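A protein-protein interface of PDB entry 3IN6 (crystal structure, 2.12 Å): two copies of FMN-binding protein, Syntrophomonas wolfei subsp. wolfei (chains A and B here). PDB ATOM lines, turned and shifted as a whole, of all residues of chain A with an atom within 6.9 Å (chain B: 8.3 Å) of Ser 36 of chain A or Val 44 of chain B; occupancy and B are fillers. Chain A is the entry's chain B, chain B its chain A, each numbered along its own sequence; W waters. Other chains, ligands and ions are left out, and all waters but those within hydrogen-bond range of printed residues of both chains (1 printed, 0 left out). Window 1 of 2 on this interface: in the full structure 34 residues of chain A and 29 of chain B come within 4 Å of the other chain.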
ATOM      1  N   THR A  34      20.184   3.149  32.324  1.00  0.00           N
ATOM      2  CA  THR A  34      20.323   1.847  31.699  1.00  0.00           C
ATOM      3  C   THR A  34      20.789   1.955  30.270  1.00  0.00           C
ATOM      4  O   THR A  34      20.724   3.018  29.659  1.00  0.00           O
ATOM      5  CB  THR A  34      18.983   1.090  31.695  1.00  0.00           C
ATOM      6  OG1 THR A  34      18.022   1.779  30.864  1.00  0.00           O
ATOM      7  CG2 THR A  34      18.457   0.960  33.126  1.00  0.00           C
ATOM      8  N   LEU A  35      21.274   0.828  29.766  1.00  0.00           N
ATOM      9  CA  LEU A  35      21.702   0.679  28.396  1.00  0.00           C
ATOM     10  C   LEU A  35      21.057  -0.594  27.895  1.00  0.00           C
ATOM     11  O   LEU A  35      21.213  -1.637  28.526  1.00  0.00           O
ATOM     12  CB  LEU A  35      23.220   0.543  28.317  1.00  0.00           C
ATOM     13  CG  LEU A  35      23.771   0.330  26.902  1.00  0.00           C
ATOM     14  CD1 LEU A  35      23.336   1.494  26.000  1.00  0.00           C
ATOM     15  CD2 LEU A  35      25.289   0.198  26.923  1.00  0.00           C
ATOM     16  N   SER A  36      20.315  -0.508  26.791  1.00  0.00           N
ATOM     17  CA  SER A  36      19.680  -1.681  26.189  1.00  0.00           C
ATOM     18  C   SER A  36      20.439  -2.053  24.932  1.00  0.00           C
ATOM     19  O   SER A  36      20.844  -1.181  24.168  1.00  0.00           O
ATOM     20  CB  SER A  36      18.220  -1.425  25.867  1.00  0.00           C
ATOM     21  OG  SER A  36      17.553  -0.989  27.026  1.00  0.00           O
ATOM     22  N   THR A  37      20.621  -3.352  24.736  1.00  0.00           N
ATOM     23  CA  THR A  37      21.435  -3.887  23.655  1.00  0.00           C
ATOM     24  C   THR A  37      20.775  -5.125  23.046  1.00  0.00           C
ATOM     25  O   THR A  37      19.722  -5.552  23.511  1.00  0.00           O
ATOM     26  CB  THR A  37      22.823  -4.241  24.186  1.00  0.00           C
ATOM     27  OG1 THR A  37      22.696  -5.163  25.292  1.00  0.00           O
ATOM     28  CG2 THR A  37      23.542  -2.969  24.653  1.00  0.00           C
ATOM     29  N   VAL A  38      21.383  -5.690  22.007  1.00  0.00           N
ATOM     30  CA  VAL A  38      20.803  -6.859  21.365  1.00  0.00           C
ATOM     31  C   VAL A  38      21.875  -7.733  20.709  1.00  0.00           C
ATOM     32  O   VAL A  38      22.876  -7.215  20.205  1.00  0.00           O
ATOM     33  CB  VAL A  38      19.758  -6.427  20.306  1.00  0.00           C
ATOM     34  CG1 VAL A  38      20.427  -5.609  19.225  1.00  0.00           C
ATOM     35  CG2 VAL A  38      19.019  -7.643  19.698  1.00  0.00           C
ATOM     36  N   VAL A  44      17.078  -9.210  23.230  1.00  0.00           N
ATOM     37  CA  VAL A  44      17.327  -7.877  23.781  1.00  0.00           C
ATOM     38  C   VAL A  44      17.762  -7.996  25.244  1.00  0.00           C
ATOM     39  O   VAL A  44      17.257  -8.845  25.999  1.00  0.00           O
ATOM     40  CB  VAL A  44      16.079  -6.988  23.686  1.00  0.00           C
ATOM     41  CG1 VAL A  44      16.410  -5.536  24.071  1.00  0.00           C
ATOM     42  CG2 VAL A  44      15.499  -7.052  22.280  1.00  0.00           C
ATOM     43  N   ASN A  45      18.707  -7.142  25.633  1.00  0.00           N
ATOM     44  CA  ASN A  45      19.177  -7.079  27.002  1.00  0.00           C
ATOM     45  C   ASN A  45      19.108  -5.637  27.466  1.00  0.00           C
ATOM     46  O   ASN A  45      19.009  -4.713  26.651  1.00  0.00           O
ATOM     47  CB  ASN A  45      20.626  -7.573  27.073  1.00  0.00           C
ATOM     48  CG  ASN A  45      21.083  -7.923  28.483  1.00  0.00           C
ATOM     49  OD1 ASN A  45      20.307  -8.396  29.304  1.00  0.00           O
ATOM     50  ND2 ASN A  45      22.380  -7.733  28.747  1.00  0.00           N
ATOM     51  N   ILE A  46      19.121  -5.467  28.783  1.00  0.00           N
ATOM     52  CA  ILE A  46      19.177  -4.165  29.443  1.00  0.00           C
ATOM     53  C   ILE A  46      19.986  -4.349  30.741  1.00  0.00           C
ATOM     54  O   ILE A  46      19.877  -5.363  31.423  1.00  0.00           O
ATOM     55  CB  ILE A  46      17.765  -3.576  29.734  1.00  0.00           C
ATOM     56  CG1 ILE A  46      17.875  -2.281  30.562  1.00  0.00           C
ATOM     57  CG2 ILE A  46      16.898  -4.603  30.459  1.00  0.00           C
ATOM     58  CD1 ILE A  46      16.561  -1.496  30.727  1.00  0.00           C
ATOM     59  N   ALA A  47      20.824  -3.376  31.057  1.00  0.00           N
ATOM     60  CA  ALA A  47      21.608  -3.424  32.273  1.00  0.00           C
ATOM     61  C   ALA A  47      21.779  -2.028  32.786  1.00  0.00           C
ATOM     62  O   ALA A  47      21.734  -1.070  32.016  1.00  0.00           O
ATOM     63  CB  ALA A  47      22.989  -4.070  32.023  1.00  0.00           C
ATOM     64  N   THR A  70      26.043  -7.285  27.850  1.00  0.00           N
ATOM     65  CA  THR A  70      25.912  -5.978  27.224  1.00  0.00           C
ATOM     66  C   THR A  70      27.089  -5.697  26.303  1.00  0.00           C
ATOM     67  O   THR A  70      26.905  -5.221  25.186  1.00  0.00           O
ATOM     68  CB  THR A  70      25.844  -4.871  28.279  1.00  0.00           C
ATOM     69  OG1 THR A  70      24.614  -4.990  28.999  1.00  0.00           O
ATOM     70  CG2 THR A  70      25.926  -3.476  27.620  1.00  0.00           C
ATOM     71  N   ASN A  73      26.979  -8.077  23.253  1.00  0.00           N
ATOM     72  CA  ASN A  73      25.958  -7.595  22.311  1.00  0.00           C
ATOM     73  C   ASN A  73      26.491  -6.454  21.442  1.00  0.00           C
ATOM     74  O   ASN A  73      26.382  -6.492  20.212  1.00  0.00           O
ATOM     75  CB  ASN A  73      24.708  -7.135  23.067  1.00  0.00           C
ATOM     76  CG  ASN A  73      23.917  -8.279  23.647  1.00  0.00           C
ATOM     77  OD1 ASN A  73      24.167  -9.444  23.347  1.00  0.00           O
ATOM     78  ND2 ASN A  73      22.919  -7.951  24.454  1.00  0.00           N
ATOM     79  N   LEU A  74      27.107  -5.464  22.083  1.00  0.00           N
ATOM     80  CA  LEU A  74      27.667  -4.321  21.372  1.00  0.00           C
ATOM     81  C   LEU A  74      28.718  -4.729  20.339  1.00  0.00           C
ATOM     82  O   LEU A  74      28.761  -4.162  19.253  1.00  0.00           O
ATOM     83  CB  LEU A  74      28.233  -3.295  22.357  1.00  0.00           C
ATOM     84  CG  LEU A  74      27.167  -2.577  23.193  1.00  0.00           C
ATOM     85  CD1 LEU A  74      27.802  -1.857  24.391  1.00  0.00           C
ATOM     86  CD2 LEU A  74      26.316  -1.606  22.334  1.00  0.00           C
ATOM     87  N   THR A  77      26.378  -6.551  17.438  1.00  0.00           N
ATOM     88  CA  THR A  77      25.438  -5.687  16.692  1.00  0.00           C
ATOM     89  C   THR A  77      25.712  -4.183  16.740  1.00  0.00           C
ATOM     90  O   THR A  77      25.211  -3.437  15.897  1.00  0.00           O
ATOM     91  CB  THR A  77      23.981  -5.926  17.156  1.00  0.00           C
ATOM     92  OG1 THR A  77      23.846  -5.561  18.545  1.00  0.00           O
ATOM     93  CG2 THR A  77      23.604  -7.387  16.961  1.00  0.00           C
ATOM     94  N   LYS A  79      24.522  -1.625  18.185  1.00  0.00           N
ATOM     95  CA  LYS A  79      23.474  -0.645  18.487  1.00  0.00           C
ATOM     96  C   LYS A  79      22.941  -0.747  19.905  1.00  0.00           C
ATOM     97  O   LYS A  79      22.888  -1.826  20.480  1.00  0.00           O
ATOM     98  CB  LYS A  79      22.326  -0.783  17.483  1.00  0.00           C
ATOM     99  CG  LYS A  79      22.825  -0.762  16.035  1.00  0.00           C
ATOM    100  CD  LYS A  79      21.709  -0.643  15.052  1.00  0.00           C
ATOM    101  CE  LYS A  79      22.164  -0.894  13.635  1.00  0.00           C
ATOM    102  NZ  LYS A  79      21.025  -0.653  12.721  1.00  0.00           N
ATOM    103  N   GLY A  80      22.536   0.391  20.457  1.00  0.00           N
ATOM    104  CA  GLY A  80      21.982   0.440  21.809  1.00  0.00           C
ATOM    105  C   GLY A  80      21.228   1.722  22.099  1.00  0.00           C
ATOM    106  O   GLY A  80      21.107   2.590  21.237  1.00  0.00           O
ATOM    107  N   VAL A  81      20.664   1.818  23.296  1.00  0.00           N
ATOM    108  CA  VAL A  81      19.991   3.040  23.725  1.00  0.00           C
ATOM    109  C   VAL A  81      20.114   3.201  25.224  1.00  0.00           C
ATOM    110  O   VAL A  81      19.863   2.250  25.983  1.00  0.00           O
ATOM    111  CB  VAL A  81      18.484   3.107  23.334  1.00  0.00           C
ATOM    112  CG1 VAL A  81      17.715   1.807  23.743  1.00  0.00           C
ATOM    113  CG2 VAL A  81      17.836   4.339  23.968  1.00  0.00           C
ATOM    114  N   PHE A  82      20.509   4.408  25.638  1.00  0.00           N
ATOM    115  CA  PHE A  82      20.622   4.762  27.046  1.00  0.00           C
ATOM    116  C   PHE A  82      19.336   5.432  27.492  1.00  0.00           C
ATOM    117  O   PHE A  82      18.756   6.229  26.731  1.00  0.00           O
ATOM    118  CB  PHE A  82      21.742   5.783  27.295  1.00  0.00           C
ATOM    119  CG  PHE A  82      23.136   5.213  27.258  1.00  0.00           C
ATOM    120  CD1 PHE A  82      23.638   4.513  28.343  1.00  0.00           C
ATOM    121  CD2 PHE A  82      23.968   5.450  26.180  1.00  0.00           C
ATOM    122  CE1 PHE A  82      24.901   3.997  28.318  1.00  0.00           C
ATOM    123  CE2 PHE A  82      25.252   4.950  26.160  1.00  0.00           C
ATOM    124  CZ  PHE A  82      25.718   4.221  27.223  1.00  0.00           C
ATOM    125  N   MET A  83      18.902   5.142  28.718  1.00  0.00           N
ATOM    126  CA  MET A  83      17.776   5.856  29.307  1.00  0.00           C
ATOM    127  C   MET A  83      18.093   6.295  30.728  1.00  0.00           C
ATOM    128  O   MET A  83      18.614   5.504  31.513  1.00  0.00           O
ATOM    129  CB  MET A  83      16.528   4.994  29.383  1.00  0.00           C
ATOM    130  CG  MET A  83      15.266   5.837  29.470  1.00  0.00           C
ATOM    131  SD  MET A  83      13.759   4.847  30.083  1.00  0.00           S
ATOM    132  CE  MET A  83      12.455   5.651  28.905  1.00  0.00           C
ATOM    133  N   TYR A  99      19.909   7.282  21.834  1.00  0.00           N
ATOM    134  CA  TYR A  99      20.129   6.133  20.949  1.00  0.00           C
ATOM    135  C   TYR A  99      21.553   6.202  20.458  1.00  0.00           C
ATOM    136  O   TYR A  99      21.992   7.252  19.995  1.00  0.00           O
ATOM    137  CB  TYR A  99      19.124   6.170  19.800  1.00  0.00           C
ATOM    138  CG  TYR A  99      17.723   6.046  20.320  1.00  0.00           C
ATOM    139  CD1 TYR A  99      17.040   7.152  20.829  1.00  0.00           C
ATOM    140  CD2 TYR A  99      17.085   4.809  20.343  1.00  0.00           C
ATOM    141  CE1 TYR A  99      15.748   7.020  21.334  1.00  0.00           C
ATOM    142  CE2 TYR A  99      15.812   4.669  20.833  1.00  0.00           C
ATOM    143  CZ  TYR A  99      15.147   5.771  21.329  1.00  0.00           C
ATOM    144  OH  TYR A  99      13.881   5.603  21.829  1.00  0.00           O
ATOM    145  N   VAL A 100      22.263   5.077  20.540  1.00  0.00           N
ATOM    146  CA  VAL A 100      23.693   5.054  20.270  1.00  0.00           C
ATOM    147  C   VAL A 100      24.233   3.887  19.440  1.00  0.00           C
ATOM    148  O   VAL A 100      23.552   2.887  19.215  1.00  0.00           O
ATOM    149  CB  VAL A 100      24.468   5.071  21.627  1.00  0.00           C
ATOM    150  CG1 VAL A 100      24.271   6.411  22.368  1.00  0.00           C
ATOM    151  CG2 VAL A 100      24.044   3.888  22.526  1.00  0.00           C
ATOM    152  N   THR B  34      10.145  -0.517  32.421  1.00  0.00           N
ATOM    153  CA  THR B  34      10.370  -0.333  30.994  1.00  0.00           C
ATOM    154  C   THR B  34      10.350  -1.632  30.205  1.00  0.00           C
ATOM    155  O   THR B  34      10.501  -2.721  30.785  1.00  0.00           O
ATOM    156  CB  THR B  34      11.769   0.307  30.701  1.00  0.00           C
ATOM    157  OG1 THR B  34      12.818  -0.623  31.048  1.00  0.00           O
ATOM    158  CG2 THR B  34      11.940   1.632  31.424  1.00  0.00           C
ATOM    159  N   LEU B  35      10.182  -1.494  28.885  1.00  0.00           N
ATOM    160  CA  LEU B  35      10.194  -2.627  27.934  1.00  0.00           C
ATOM    161  C   LEU B  35      11.162  -2.242  26.802  1.00  0.00           C
ATOM    162  O   LEU B  35      10.957  -1.249  26.093  1.00  0.00           O
ATOM    163  CB  LEU B  35       8.790  -2.935  27.392  1.00  0.00           C
ATOM    164  CG  LEU B  35       8.696  -3.978  26.242  1.00  0.00           C
ATOM    165  CD1 LEU B  35       9.287  -5.308  26.698  1.00  0.00           C
ATOM    166  CD2 LEU B  35       7.226  -4.183  25.760  1.00  0.00           C
ATOM    167  N   SER B  36      12.242  -3.001  26.667  1.00  0.00           N
ATOM    168  CA  SER B  36      13.221  -2.729  25.650  1.00  0.00           C
ATOM    169  C   SER B  36      12.910  -3.710  24.519  1.00  0.00           C
ATOM    170  O   SER B  36      12.654  -4.887  24.779  1.00  0.00           O
ATOM    171  CB  SER B  36      14.655  -2.891  26.197  1.00  0.00           C
ATOM    172  OG  SER B  36      14.920  -1.977  27.244  1.00  0.00           O
ATOM    173  N   THR B  37      12.912  -3.205  23.286  1.00  0.00           N
ATOM    174  CA  THR B  37      12.587  -3.983  22.070  1.00  0.00           C
ATOM    175  C   THR B  37      13.625  -3.738  20.982  1.00  0.00           C
ATOM    176  O   THR B  37      14.537  -2.958  21.185  1.00  0.00           O
ATOM    177  CB  THR B  37      11.170  -3.611  21.546  1.00  0.00           C
ATOM    178  OG1 THR B  37      11.109  -2.205  21.232  1.00  0.00           O
ATOM    179  CG2 THR B  37      10.078  -3.961  22.609  1.00  0.00           C
ATOM    180  N   VAL B  38      13.488  -4.420  19.836  1.00  0.00           N
ATOM    181  CA  VAL B  38      14.416  -4.303  18.717  1.00  0.00           C
ATOM    182  C   VAL B  38      13.697  -4.570  17.391  1.00  0.00           C
ATOM    183  O   VAL B  38      12.700  -5.286  17.384  1.00  0.00           O
ATOM    184  CB  VAL B  38      15.578  -5.345  18.831  1.00  0.00           C
ATOM    185  CG1 VAL B  38      15.047  -6.760  18.703  1.00  0.00           C
ATOM    186  CG2 VAL B  38      16.663  -5.089  17.776  1.00  0.00           C
ATOM    187  N   ASP B  39      14.187  -3.976  16.291  1.00  0.00           N
ATOM    188  CA  ASP B  39      13.636  -4.245  14.951  1.00  0.00           C
ATOM    189  C   ASP B  39      14.565  -5.170  14.171  1.00  0.00           C
ATOM    190  O   ASP B  39      15.629  -5.543  14.687  1.00  0.00           O
ATOM    191  CB  ASP B  39      13.324  -2.962  14.150  1.00  0.00           C
ATOM    192  CG  ASP B  39      14.565  -2.270  13.566  1.00  0.00           C
ATOM    193  OD1 ASP B  39      15.728  -2.650  13.837  1.00  0.00           O
ATOM    194  OD2 ASP B  39      14.351  -1.316  12.798  1.00  0.00           O
ATOM    195  N   ARG B  40      14.155  -5.509  12.933  1.00  0.00           N
ATOM    196  CA  ARG B  40      14.874  -6.438  12.056  1.00  0.00           C
ATOM    197  C   ARG B  40      16.306  -5.997  11.712  1.00  0.00           C
ATOM    198  O   ARG B  40      17.136  -6.821  11.303  1.00  0.00           O
ATOM    199  CB  ARG B  40      14.093  -6.660  10.730  1.00  0.00           C
ATOM    200  CG  ARG B  40      13.862  -5.350   9.993  1.00  0.00           C
ATOM    201  CD  ARG B  40      13.677  -5.398   8.490  1.00  0.00           C
ATOM    202  NE  ARG B  40      12.305  -5.625   8.102  1.00  0.00           N
ATOM    203  CZ  ARG B  40      11.699  -5.098   7.037  1.00  0.00           C
ATOM    204  NH1 ARG B  40      12.298  -4.241   6.221  1.00  0.00           N
ATOM    205  NH2 ARG B  40      10.435  -5.419   6.815  1.00  0.00           N
ATOM    206  N   ASN B  41      16.563  -4.692  11.805  1.00  0.00           N
ATOM    207  CA  ASN B  41      17.886  -4.133  11.538  1.00  0.00           C
ATOM    208  C   ASN B  41      18.737  -3.936  12.788  1.00  0.00           C
ATOM    209  O   ASN B  41      19.757  -3.252  12.727  1.00  0.00           O
ATOM    210  CB  ASN B  41      17.780  -2.813  10.778  1.00  0.00           C
ATOM    211  CG  ASN B  41      17.956  -2.983   9.307  1.00  0.00           C
ATOM    212  OD1 ASN B  41      17.263  -3.783   8.658  1.00  0.00           O
ATOM    213  ND2 ASN B  41      18.894  -2.225   8.750  1.00  0.00           N
ATOM    214  N   TYR B  42      18.301  -4.524  13.902  1.00  0.00           N
ATOM    215  CA  TYR B  42      19.002  -4.484  15.182  1.00  0.00           C
ATOM    216  C   TYR B  42      18.905  -3.149  15.929  1.00  0.00           C
ATOM    217  O   TYR B  42      19.605  -2.939  16.926  1.00  0.00           O
ATOM    218  CB  TYR B  42      20.475  -4.945  15.029  1.00  0.00           C
ATOM    219  CG  TYR B  42      20.596  -6.367  14.512  1.00  0.00           C
ATOM    220  CD1 TYR B  42      20.252  -7.443  15.320  1.00  0.00           C
ATOM    221  CD2 TYR B  42      21.043  -6.636  13.226  1.00  0.00           C
ATOM    222  CE1 TYR B  42      20.335  -8.743  14.862  1.00  0.00           C
ATOM    223  CE2 TYR B  42      21.138  -7.951  12.762  1.00  0.00           C
ATOM    224  CZ  TYR B  42      20.779  -8.992  13.589  1.00  0.00           C
ATOM    225  OH  TYR B  42      20.868 -10.298  13.161  1.00  0.00           O
ATOM    226  N   GLU B  43      18.019  -2.260  15.474  1.00  0.00           N
ATOM    227  CA  GLU B  43      17.843  -0.957  16.122  1.00  0.00           C
ATOM    228  C   GLU B  43      17.040  -1.214  17.398  1.00  0.00           C
ATOM    229  O   GLU B  43      15.927  -1.743  17.349  1.00  0.00           O
ATOM    230  CB  GLU B  43      17.144   0.044  15.177  1.00  0.00           C
ATOM    231  N   VAL B  44      17.619  -0.862  18.540  1.00  0.00           N
ATOM    232  CA  VAL B  44      16.996  -1.121  19.829  1.00  0.00           C
ATOM    233  C   VAL B  44      16.209   0.092  20.310  1.00  0.00           C
ATOM    234  O   VAL B  44      16.611   1.231  20.106  1.00  0.00           O
ATOM    235  CB  VAL B  44      18.074  -1.490  20.892  1.00  0.00           C
ATOM    236  CG1 VAL B  44      17.445  -1.779  22.244  1.00  0.00           C
ATOM    237  CG2 VAL B  44      18.897  -2.683  20.425  1.00  0.00           C
ATOM    238  N   ASN B  45      15.062  -0.169  20.913  1.00  0.00           N
ATOM    239  CA  ASN B  45      14.246   0.867  21.521  1.00  0.00           C
ATOM    240  C   ASN B  45      13.974   0.473  22.954  1.00  0.00           C
ATOM    241  O   ASN B  45      14.095  -0.702  23.323  1.00  0.00           O
ATOM    242  CB  ASN B  45      12.896   1.010  20.800  1.00  0.00           C
ATOM    243  CG  ASN B  45      12.156   2.294  21.191  1.00  0.00           C
ATOM    244  OD1 ASN B  45      12.778   3.332  21.352  1.00  0.00           O
ATOM    245  ND2 ASN B  45      10.830   2.222  21.334  1.00  0.00           N
ATOM    246  N   ILE B  46      13.621   1.475  23.745  1.00  0.00           N
ATOM    247  CA  ILE B  46      13.177   1.323  25.120  1.00  0.00           C
ATOM    248  C   ILE B  46      12.042   2.343  25.371  1.00  0.00           C
ATOM    249  O   ILE B  46      12.067   3.474  24.863  1.00  0.00           O
ATOM    250  CB  ILE B  46      14.305   1.504  26.120  1.00  0.00           C
ATOM    251  CG1 ILE B  46      13.788   1.205  27.538  1.00  0.00           C
ATOM    252  CG2 ILE B  46      14.925   2.893  25.985  1.00  0.00           C
ATOM    253  CD1 ILE B  46      14.841   1.162  28.581  1.00  0.00           C
ATOM    254  N   ALA B  47      11.036   1.921  26.126  1.00  0.00           N
ATOM    255  CA  ALA B  47       9.894   2.768  26.423  1.00  0.00           C
ATOM    256  C   ALA B  47       9.381   2.454  27.817  1.00  0.00           C
ATOM    257  O   ALA B  47       9.522   1.313  28.302  1.00  0.00           O
ATOM    258  CB  ALA B  47       8.782   2.539  25.380  1.00  0.00           C
ATOM    259  N   LYS B  69       6.406   2.578  18.385  1.00  0.00           N
ATOM    260  CA  LYS B  69       7.656   1.966  17.907  1.00  0.00           C
ATOM    261  C   LYS B  69       7.865   0.613  18.602  1.00  0.00           C
ATOM    262  O   LYS B  69       8.184  -0.388  17.955  1.00  0.00           O
ATOM    263  CB  LYS B  69       8.824   2.920  18.148  1.00  0.00           C
ATOM    264  CG  LYS B  69      10.205   2.566  17.545  1.00  0.00           C
ATOM    265  CD  LYS B  69      10.171   2.437  16.031  1.00  0.00           C
ATOM    266  CE  LYS B  69      11.326   3.210  15.324  1.00  0.00           C
ATOM    267  NZ  LYS B  69      12.658   2.911  15.869  1.00  0.00           N
ATOM    268  N   ASN B  73       8.197  -2.880  16.668  1.00  0.00           N
ATOM    269  CA  ASN B  73       9.340  -3.788  16.913  1.00  0.00           C
ATOM    270  C   ASN B  73       8.868  -5.207  17.294  1.00  0.00           C
ATOM    271  O   ASN B  73       9.275  -6.226  16.674  1.00  0.00           O
ATOM    272  CB  ASN B  73      10.241  -3.216  17.993  1.00  0.00           C
ATOM    273  CG  ASN B  73      11.070  -2.041  17.497  1.00  0.00           C
ATOM    274  OD1 ASN B  73      11.194  -1.811  16.294  1.00  0.00           O
ATOM    275  ND2 ASN B  73      11.664  -1.312  18.424  1.00  0.00           N
ATOM    276  N   VAL B  81      12.545  -7.242  26.634  1.00  0.00           N
ATOM    277  CA  VAL B  81      12.894  -7.437  28.022  1.00  0.00           C
ATOM    278  C   VAL B  81      12.315  -6.331  28.882  1.00  0.00           C
ATOM    279  O   VAL B  81      12.531  -5.149  28.619  1.00  0.00           O
ATOM    280  CB  VAL B  81      14.433  -7.532  28.271  1.00  0.00           C
ATOM    281  CG1 VAL B  81      15.199  -6.264  27.772  1.00  0.00           C
ATOM    282  CG2 VAL B  81      14.699  -7.798  29.761  1.00  0.00           C
ATOM    283  N   MET B  83      12.065  -4.433  32.492  1.00  0.00           N
ATOM    284  CA  MET B  83      12.878  -4.191  33.643  1.00  0.00           C
ATOM    285  C   MET B  83      12.120  -3.295  34.577  1.00  0.00           C
ATOM    286  O   MET B  83      11.514  -2.318  34.145  1.00  0.00           O
ATOM    287  CB  MET B  83      14.218  -3.521  33.331  1.00  0.00           C
ATOM    288  CG  MET B  83      14.997  -3.186  34.664  1.00  0.00           C
ATOM    289  SD  MET B  83      16.777  -2.474  34.524  1.00  0.00           S
ATOM    290  CE  MET B  83      17.846  -4.069  34.508  1.00  0.00           C
HETATM  291  O   HOH W   1      19.228   1.533  19.110  1.00  0.00           O
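The side-chain hydroxyl of Ser 36 of chain A lies within hydrogen-bond range of the side-chain hydroxyl of Ser 36 of chain B (2.8 Å). O of Asn 41 of chain B is in hydrogen-bond range of NZ of Lys 79 of chain A (2.9 Å). The side-chain hydroxyl of Tyr 99 of chain A lies within hydrogen-bond range of the side-chain amide oxygen of Asn 45 of chain B (2.6 Å).
The backbone NH of Ser 36 of chain B lies within hydrogen-bond range of the backbone carbonyl oxygen of Val 81 of chain B (2.9 Å). N of Asn 41 of chain B sits at hydrogen-bond distance from OD1 of Asp 39 of chain B, at 3.0 Å. N of Tyr 42 of chain B is in hydrogen-bond range of OD1 of Asp 39 of chain B, at 3.2 Å. N of Thr 34 of chain A lies within hydrogen-bond range of O of Met 83 of chain A (2.9 Å). The backbone carbonyl oxygen of Thr 37 of chain A sits at hydrogen-bond distance from the backbone NH of Asn 45 of chain A. The backbone carbonyl oxygen (O) of Val 38 of chain A is in hydrogen-bond range of the side-chain hydroxyl (OG1) of Thr 77 of chain A, 2.5 Å away.
Among the printed residues, merely in contact across the chains: Thr 34 of chain A with Ile 46 of chain B, Ser 36 of chain A with Val 44 of chain B, Ser 36 of chain A with Ile 46 of chain B, Val 38 of chain A with Val 38 of chain B, Val 38 of chain A with Tyr 42 of chain B, Val 38 of chain A with Val 44 of chain B, Val 44 of chain A with Ser 36 of chain B, Val 44 of chain A with Val 38 of chain B, Val 44 of chain A with Val 81 of chain B, Asn 45 of chain A with Val 81 of chain B, Ile 46 of chain A with Thr 34 of chain B, Ile 46 of chain A with Ser 36 of chain B, Ile 46 of chain A with Ile 46 of chain B, Ile 46 of chain A with Val 81 of chain B, Ile 46 of chain A with Met 83 of chain B, Thr 77 of chain A with Tyr 42 of chain B, Lys 79 of chain A with Tyr 42 of chain B, Val 81 of chain A with Val 44 of chain B, Val 81 of chain A with Ile 46 of chain B, Met 83 of chain A with Thr 34 of chain B and Tyr 99 of chain A with Val 44 of chain B.
Ser 36 of chain A touches just these residues of chain B: Ser 36 (2.8 Å), Val 44 (3.7 Å) and Ile 46 (3.8 Å). Of chain A, only Ser 36, Val 38, Val 81 and Tyr 99 come within 4 Å of Val 44 of chain B. No residue of chain B comes within 4 Å of Thr 37 of chain A. Of the printed residues of chain B, Thr 34 of chain A touches Ile 46. Of the printed residues of chain B, Val 44 of chain A touches Ser 36, Val 38 and Val 81. Of the printed residues of chain A, Thr 34 of chain B touches Ile 46 (3.9 Å) and Met 83 (3.9 Å). Printed residues of chain B within 4 Å of Lys 79 of chain A: Asn 41 and Tyr 42. Printed residues of chain A within 4 Å of Tyr 42 of chain B: Val 38, Thr 77 and Lys 79. Glu 43 of chain B touches none of the printed residues of chain A. The nearest residue of chain B that does not touch Ser 36 of chain A is Asn 45 of chain B (4.9 Å). The nearest residue of chain A that does not touch Val 44 of chain B is Thr 37 of chain A (4.04 Å).
Hydrophobic or aromatic side chains of chain A that line the printed part of chain B: Val 38, Val 44, Ile 46, Val 81, Met 83 and Tyr 99. Among the printed residues, 24 pairs touch across the chains.
Val 38 of chain A touches its own counterpart, Val 38 of chain B. Asn 45 of chain A touches Val 81 of chain B, but with the chains exchanged Val 81 of chain A does not touch Asn 45 of chain B (4.05 Å). Ile 46 of chain B touches its own counterpart, Ile 46 of chain A. Ile 46 of chain A touches Met 83 of chain B, but with the chains exchanged Met 83 of chain A does not touch Ile 46 of chain B (4.1 Å). Positions printed for both chains: 34, 35, 36, 37, 38, 44, 45, 46, 47, 73, 81 and 83. Of the 24 pairs that touch across the chains among the printed residues, 15 have their exchanged pair printed and touching as well.
Water W1 lies within hydrogen-bond range of O of Val 44 of chain B and O of Gly 80 of chain A.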
